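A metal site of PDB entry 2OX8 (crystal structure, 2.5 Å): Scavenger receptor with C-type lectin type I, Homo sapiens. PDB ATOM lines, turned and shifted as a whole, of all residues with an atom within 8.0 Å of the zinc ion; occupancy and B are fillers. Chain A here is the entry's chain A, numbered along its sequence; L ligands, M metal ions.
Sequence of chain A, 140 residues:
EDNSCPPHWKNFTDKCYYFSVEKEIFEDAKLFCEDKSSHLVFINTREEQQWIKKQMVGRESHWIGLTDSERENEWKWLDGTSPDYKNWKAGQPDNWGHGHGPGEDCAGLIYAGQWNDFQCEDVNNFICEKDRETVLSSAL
The side-chain hydroxyl (OH) of Tyr 17 lies close to the side-chain carboxylate (OE1) of Glu 48 (2.6 Å).
The side-chain carboxylate (OE2) of Glu 48 lies within hydrogen-bond range of the backbone NH (N) of Asn 44, at 3.1 Å.
The backbone NH (N) of Glu 129 is in hydrogen-bond range of the backbone carbonyl oxygen (O) of His 39 (2.9 Å).
The side-chain hydroxyl (OG1) of Thr 45 lies within hydrogen-bond range of the backbone NH (N) of Glu 48, 3.3 Å away.
The side-chain hydroxyl (OH) of Tyr 17 lies close to the side-chain carboxylate (OE2) of Glu 129.
Residues that only touch the zinc ion: Tyr 17.
Within 4 Å of the zinc ion: Tyr 17, Phe 42, Glu 48 and Glu 129.
The nearest printed residue that does not touch the zinc ion is Lys 15 (4.1 Å).
The zinc ion is bound by the side-chain carboxylate (OE2) of Glu 129 (1.9 Å), the side-chain carboxylate (OE1) of Glu 48 (2.0 Å), a chlorine (CL1) of the ligand (2.1 Å) and the backbone carbonyl oxygen (O) of Phe 42 (2.1 Å).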
ATOM      1  N   PHE A  12      14.757 -27.354 -25.706  1.00  0.00           N
ATOM      2  CA  PHE A  12      14.180 -28.119 -24.614  1.00  0.00           C
ATOM      3  C   PHE A  12      12.804 -28.508 -25.108  1.00  0.00           C
ATOM      4  O   PHE A  12      11.985 -27.652 -25.439  1.00  0.00           O
ATOM      5  CB  PHE A  12      14.025 -27.254 -23.355  1.00  0.00           C
ATOM      6  CG  PHE A  12      13.292 -27.957 -22.231  1.00  0.00           C
ATOM      7  CD1 PHE A  12      13.934 -28.903 -21.445  1.00  0.00           C
ATOM      8  CD2 PHE A  12      11.947 -27.677 -21.991  1.00  0.00           C
ATOM      9  CE1 PHE A  12      13.259 -29.577 -20.422  1.00  0.00           C
ATOM     10  CE2 PHE A  12      11.262 -28.346 -20.977  1.00  0.00           C
ATOM     11  CZ  PHE A  12      11.923 -29.298 -20.193  1.00  0.00           C
ATOM     12  N   ASP A  14      10.168 -29.105 -27.528  1.00  0.00           N
ATOM     13  CA  ASP A  14      10.008 -28.720 -28.935  1.00  0.00           C
ATOM     14  C   ASP A  14      10.158 -27.213 -29.104  1.00  0.00           C
ATOM     15  O   ASP A  14       9.722 -26.641 -30.103  1.00  0.00           O
ATOM     16  CB  ASP A  14       8.637 -29.161 -29.448  1.00  0.00           C
ATOM     17  CG  ASP A  14       7.490 -28.409 -28.806  1.00  0.00           C
ATOM     18  OD1 ASP A  14       7.634 -27.930 -27.656  1.00  0.00           O
ATOM     19  OD2 ASP A  14       6.418 -28.307 -29.441  1.00  0.00           O
ATOM     20  N   LYS A  15      10.800 -26.588 -28.129  1.00  0.00           N
ATOM     21  CA  LYS A  15      10.950 -25.146 -28.146  1.00  0.00           C
ATOM     22  C   LYS A  15      12.388 -24.632 -28.113  1.00  0.00           C
ATOM     23  O   LYS A  15      13.281 -25.210 -27.455  1.00  0.00           O
ATOM     24  CB  LYS A  15      10.202 -24.550 -26.960  1.00  0.00           C
ATOM     25  CG  LYS A  15       8.796 -25.069 -26.812  1.00  0.00           C
ATOM     26  CD  LYS A  15       8.195 -24.641 -25.493  1.00  0.00           C
ATOM     27  CE  LYS A  15       6.719 -24.899 -25.479  1.00  0.00           C
ATOM     28  NZ  LYS A  15       6.505 -26.337 -25.649  1.00  0.00           N
ATOM     29  N   TYR A  17      14.790 -21.533 -27.118  1.00  0.00           N
ATOM     30  CA  TYR A  17      14.872 -20.426 -26.170  1.00  0.00           C
ATOM     31  C   TYR A  17      16.057 -19.505 -26.466  1.00  0.00           C
ATOM     32  O   TYR A  17      17.108 -19.932 -26.913  1.00  0.00           O
ATOM     33  CB  TYR A  17      14.991 -20.970 -24.747  1.00  0.00           C
ATOM     34  CG  TYR A  17      13.821 -21.795 -24.283  1.00  0.00           C
ATOM     35  CD1 TYR A  17      13.614 -23.072 -24.762  1.00  0.00           C
ATOM     36  CD2 TYR A  17      12.894 -21.272 -23.381  1.00  0.00           C
ATOM     37  CE1 TYR A  17      12.510 -23.824 -24.351  1.00  0.00           C
ATOM     38  CE2 TYR A  17      11.785 -22.000 -22.976  1.00  0.00           C
ATOM     39  CZ  TYR A  17      11.607 -23.286 -23.459  1.00  0.00           C
ATOM     40  OH  TYR A  17      10.526 -24.036 -23.029  1.00  0.00           O
ATOM     41  N   HIS A  39       8.200 -14.839 -28.416  1.00  0.00           N
ATOM     42  CA  HIS A  39       7.626 -13.982 -27.412  1.00  0.00           C
ATOM     43  C   HIS A  39       8.332 -14.268 -26.109  1.00  0.00           C
ATOM     44  O   HIS A  39       8.926 -15.335 -25.961  1.00  0.00           O
ATOM     45  CB  HIS A  39       6.146 -14.327 -27.229  1.00  0.00           C
ATOM     46  CG  HIS A  39       5.891 -15.792 -27.075  1.00  0.00           C
ATOM     47  ND1 HIS A  39       6.235 -16.494 -25.939  1.00  0.00           N
ATOM     48  CD2 HIS A  39       5.392 -16.704 -27.948  1.00  0.00           C
ATOM     49  CE1 HIS A  39       5.959 -17.777 -26.109  1.00  0.00           C
ATOM     50  NE2 HIS A  39       5.448 -17.930 -27.319  1.00  0.00           N
ATOM     51  N   LEU A  40       8.287 -13.309 -25.188  1.00  0.00           N
ATOM     52  CA  LEU A  40       8.898 -13.512 -23.905  1.00  0.00           C
ATOM     53  C   LEU A  40       8.355 -14.878 -23.428  1.00  0.00           C
ATOM     54  O   LEU A  40       7.163 -15.204 -23.579  1.00  0.00           O
ATOM     55  CB  LEU A  40       8.544 -12.349 -22.977  1.00  0.00           C
ATOM     56  CG  LEU A  40       9.365 -11.054 -23.242  1.00  0.00           C
ATOM     57  CD1 LEU A  40       8.683  -9.844 -22.627  1.00  0.00           C
ATOM     58  CD2 LEU A  40      10.787 -11.214 -22.683  1.00  0.00           C
ATOM     59  N   VAL A  41       9.277 -15.678 -22.892  1.00  0.00           N
ATOM     60  CA  VAL A  41       9.018 -17.029 -22.434  1.00  0.00           C
ATOM     61  C   VAL A  41       7.791 -17.233 -21.512  1.00  0.00           C
ATOM     62  O   VAL A  41       7.466 -16.378 -20.690  1.00  0.00           O
ATOM     63  CB  VAL A  41      10.283 -17.566 -21.725  1.00  0.00           C
ATOM     64  CG1 VAL A  41      10.506 -16.827 -20.424  1.00  0.00           C
ATOM     65  CG2 VAL A  41      10.184 -19.036 -21.482  1.00  0.00           C
ATOM     66  N   PHE A  42       7.116 -18.366 -21.698  1.00  0.00           N
ATOM     67  CA  PHE A  42       5.962 -18.755 -20.875  1.00  0.00           C
ATOM     68  C   PHE A  42       6.501 -19.980 -20.139  1.00  0.00           C
ATOM     69  O   PHE A  42       7.142 -20.841 -20.752  1.00  0.00           O
ATOM     70  CB  PHE A  42       4.765 -19.218 -21.710  1.00  0.00           C
ATOM     71  CG  PHE A  42       4.155 -18.166 -22.562  1.00  0.00           C
ATOM     72  CD1 PHE A  42       3.443 -18.516 -23.689  1.00  0.00           C
ATOM     73  CD2 PHE A  42       4.318 -16.818 -22.261  1.00  0.00           C
ATOM     74  CE1 PHE A  42       2.898 -17.537 -24.528  1.00  0.00           C
ATOM     75  CE2 PHE A  42       3.776 -15.831 -23.089  1.00  0.00           C
ATOM     76  CZ  PHE A  42       3.067 -16.199 -24.239  1.00  0.00           C
ATOM     77  N   ILE A  43       6.273 -20.057 -18.833  1.00  0.00           N
ATOM     78  CA  ILE A  43       6.743 -21.203 -18.069  1.00  0.00           C
ATOM     79  C   ILE A  43       5.526 -21.959 -17.549  1.00  0.00           C
ATOM     80  O   ILE A  43       4.873 -21.523 -16.601  1.00  0.00           O
ATOM     81  CB  ILE A  43       7.644 -20.744 -16.917  1.00  0.00           C
ATOM     82  CG1 ILE A  43       8.881 -20.079 -17.495  1.00  0.00           C
ATOM     83  CG2 ILE A  43       8.006 -21.919 -16.027  1.00  0.00           C
ATOM     84  CD1 ILE A  43       9.596 -19.177 -16.548  1.00  0.00           C
ATOM     85  N   ASN A  44       5.216 -23.091 -18.168  1.00  0.00           N
ATOM     86  CA  ASN A  44       4.027 -23.834 -17.790  1.00  0.00           C
ATOM     87  C   ASN A  44       4.143 -25.185 -17.075  1.00  0.00           C
ATOM     88  O   ASN A  44       3.146 -25.886 -16.928  1.00  0.00           O
ATOM     89  CB  ASN A  44       3.137 -23.992 -19.013  1.00  0.00           C
ATOM     90  CG  ASN A  44       2.544 -22.683 -19.435  1.00  0.00           C
ATOM     91  OD1 ASN A  44       1.846 -22.029 -18.660  1.00  0.00           O
ATOM     92  ND2 ASN A  44       2.810 -22.270 -20.666  1.00  0.00           N
ATOM     93  N   THR A  45       5.337 -25.528 -16.612  1.00  0.00           N
ATOM     94  CA  THR A  45       5.520 -26.780 -15.916  1.00  0.00           C
ATOM     95  C   THR A  45       6.765 -26.634 -15.088  1.00  0.00           C
ATOM     96  O   THR A  45       7.637 -25.848 -15.424  1.00  0.00           O
ATOM     97  CB  THR A  45       5.728 -27.955 -16.896  1.00  0.00           C
ATOM     98  OG1 THR A  45       6.822 -27.645 -17.779  1.00  0.00           O
ATOM     99  CG2 THR A  45       4.467 -28.203 -17.710  1.00  0.00           C
ATOM    100  N   GLU A  48       9.994 -27.495 -16.992  1.00  0.00           N
ATOM    101  CA  GLU A  48      10.494 -26.428 -17.843  1.00  0.00           C
ATOM    102  C   GLU A  48      11.220 -25.429 -16.931  1.00  0.00           C
ATOM    103  O   GLU A  48      12.354 -25.055 -17.196  1.00  0.00           O
ATOM    104  CB  GLU A  48       9.356 -25.740 -18.616  1.00  0.00           C
ATOM    105  CG  GLU A  48       9.809 -24.642 -19.580  1.00  0.00           C
ATOM    106  CD  GLU A  48       8.661 -23.938 -20.300  1.00  0.00           C
ATOM    107  OE1 GLU A  48       8.913 -23.107 -21.203  1.00  0.00           O
ATOM    108  OE2 GLU A  48       7.503 -24.198 -19.973  1.00  0.00           O
ATOM    109  N   GLN A  49      10.561 -25.031 -15.857  1.00  0.00           N
ATOM    110  CA  GLN A  49      11.142 -24.093 -14.895  1.00  0.00           C
ATOM    111  C   GLN A  49      12.500 -24.585 -14.378  1.00  0.00           C
ATOM    112  O   GLN A  49      13.420 -23.803 -14.221  1.00  0.00           O
ATOM    113  CB  GLN A  49      10.180 -23.853 -13.724  1.00  0.00           C
ATOM    114  CG  GLN A  49      10.749 -23.091 -12.546  1.00  0.00           C
ATOM    115  CD  GLN A  49      11.089 -21.657 -12.874  1.00  0.00           C
ATOM    116  OE1 GLN A  49      10.202 -20.843 -13.146  1.00  0.00           O
ATOM    117  NE2 GLN A  49      12.384 -21.324 -12.832  1.00  0.00           N
ATOM    118  N   TRP A  51      14.575 -26.481 -15.988  1.00  0.00           N
ATOM    119  CA  TRP A  51      15.513 -26.447 -17.111  1.00  0.00           C
ATOM    120  C   TRP A  51      15.992 -25.035 -17.351  1.00  0.00           C
ATOM    121  O   TRP A  51      17.176 -24.782 -17.538  1.00  0.00           O
ATOM    122  CB  TRP A  51      14.854 -26.959 -18.381  1.00  0.00           C
ATOM    123  CG  TRP A  51      15.749 -26.861 -19.570  1.00  0.00           C
ATOM    124  CD1 TRP A  51      16.774 -27.711 -19.884  1.00  0.00           C
ATOM    125  CD2 TRP A  51      15.742 -25.852 -20.596  1.00  0.00           C
ATOM    126  NE1 TRP A  51      17.393 -27.296 -21.039  1.00  0.00           N
ATOM    127  CE2 TRP A  51      16.791 -26.157 -21.500  1.00  0.00           C
ATOM    128  CE3 TRP A  51      14.945 -24.722 -20.841  1.00  0.00           C
ATOM    129  CZ2 TRP A  51      17.069 -25.364 -22.625  1.00  0.00           C
ATOM    130  CZ3 TRP A  51      15.233 -23.932 -21.958  1.00  0.00           C
ATOM    131  CH2 TRP A  51      16.289 -24.264 -22.836  1.00  0.00           C
ATOM    132  N   ILE A  52      15.034 -24.103 -17.363  1.00  0.00           N
ATOM    133  CA  ILE A  52      15.345 -22.708 -17.584  1.00  0.00           C
ATOM    134  C   ILE A  52      16.391 -22.213 -16.600  1.00  0.00           C
ATOM    135  O   ILE A  52      17.299 -21.474 -16.967  1.00  0.00           O
ATOM    136  CB  ILE A  52      14.061 -21.865 -17.496  1.00  0.00           C
ATOM    137  CG1 ILE A  52      13.263 -22.039 -18.789  1.00  0.00           C
ATOM    138  CG2 ILE A  52      14.385 -20.396 -17.257  1.00  0.00           C
ATOM    139  CD1 ILE A  52      11.907 -21.339 -18.802  1.00  0.00           C
ATOM    140  N   TRP A  77      -0.104 -14.832 -19.037  1.00  0.00           N
ATOM    141  CA  TRP A  77       0.998 -14.969 -19.966  1.00  0.00           C
ATOM    142  C   TRP A  77       0.543 -14.180 -21.190  1.00  0.00           C
ATOM    143  O   TRP A  77      -0.668 -14.078 -21.419  1.00  0.00           O
ATOM    144  CB  TRP A  77       1.183 -16.430 -20.333  1.00  0.00           C
ATOM    145  CG  TRP A  77       1.644 -17.271 -19.200  1.00  0.00           C
ATOM    146  CD1 TRP A  77       0.951 -18.286 -18.601  1.00  0.00           C
ATOM    147  CD2 TRP A  77       2.924 -17.222 -18.564  1.00  0.00           C
ATOM    148  NE1 TRP A  77       1.734 -18.869 -17.630  1.00  0.00           N
ATOM    149  CE2 TRP A  77       2.944 -18.239 -17.581  1.00  0.00           C
ATOM    150  CE3 TRP A  77       4.063 -16.414 -18.724  1.00  0.00           C
ATOM    151  CZ2 TRP A  77       4.044 -18.470 -16.767  1.00  0.00           C
ATOM    152  CZ3 TRP A  77       5.161 -16.656 -17.901  1.00  0.00           C
ATOM    153  CH2 TRP A  77       5.149 -17.671 -16.935  1.00  0.00           C
ATOM    154  N   GLU A 129      11.095 -17.193 -26.533  1.00  0.00           N
ATOM    155  CA  GLU A 129      10.700 -18.565 -26.720  1.00  0.00           C
ATOM    156  C   GLU A 129       9.811 -18.710 -27.961  1.00  0.00           C
ATOM    157  O   GLU A 129       9.096 -17.764 -28.324  1.00  0.00           O
ATOM    158  CB  GLU A 129       9.949 -19.011 -25.459  1.00  0.00           C
ATOM    159  CG  GLU A 129       9.277 -20.388 -25.503  1.00  0.00           C
ATOM    160  CD  GLU A 129       8.346 -20.622 -24.314  1.00  0.00           C
ATOM    161  OE1 GLU A 129       7.417 -19.825 -24.118  1.00  0.00           O
ATOM    162  OE2 GLU A 129       8.539 -21.619 -23.585  1.00  0.00           O
ATOM    163  N   LYS A 130       9.888 -19.867 -28.603  1.00  0.00           N
ATOM    164  CA  LYS A 130       9.051 -20.165 -29.762  1.00  0.00           C
ATOM    165  C   LYS A 130       9.003 -21.680 -29.948  1.00  0.00           C
ATOM    166  O   LYS A 130      10.021 -22.360 -29.836  1.00  0.00           O
ATOM    167  CB  LYS A 130       9.554 -19.477 -31.034  1.00  0.00           C
ATOM    168  CG  LYS A 130      10.974 -19.827 -31.444  1.00  0.00           C
ATOM    169  CD  LYS A 130      11.323 -19.111 -32.751  1.00  0.00           C
ATOM    170  CE  LYS A 130      12.823 -19.045 -33.004  1.00  0.00           C
ATOM    171  NZ  LYS A 130      13.073 -18.087 -34.119  1.00  0.00           N
ATOM    172  N   ASP A 131       7.808 -22.200 -30.203  1.00  0.00           N
ATOM    173  CA  ASP A 131       7.587 -23.622 -30.391  1.00  0.00           C
ATOM    174  C   ASP A 131       7.698 -23.966 -31.882  1.00  0.00           C
ATOM    175  O   ASP A 131       7.002 -23.398 -32.709  1.00  0.00           O
ATOM    176  CB  ASP A 131       6.193 -23.977 -29.819  1.00  0.00           C
ATOM    177  CG  ASP A 131       5.729 -25.364 -30.196  1.00  0.00           C
ATOM    178  OD1 ASP A 131       5.632 -25.680 -31.403  1.00  0.00           O
ATOM    179  OD2 ASP A 131       5.433 -26.161 -29.294  1.00  0.00           O
HETATM  180 CL1  LIG L   1       5.467 -22.972 -22.307  1.00  0.00          CL
HETATM  181 ZN    ZN M   1       7.443 -22.292 -22.246  1.00  0.00          ZN
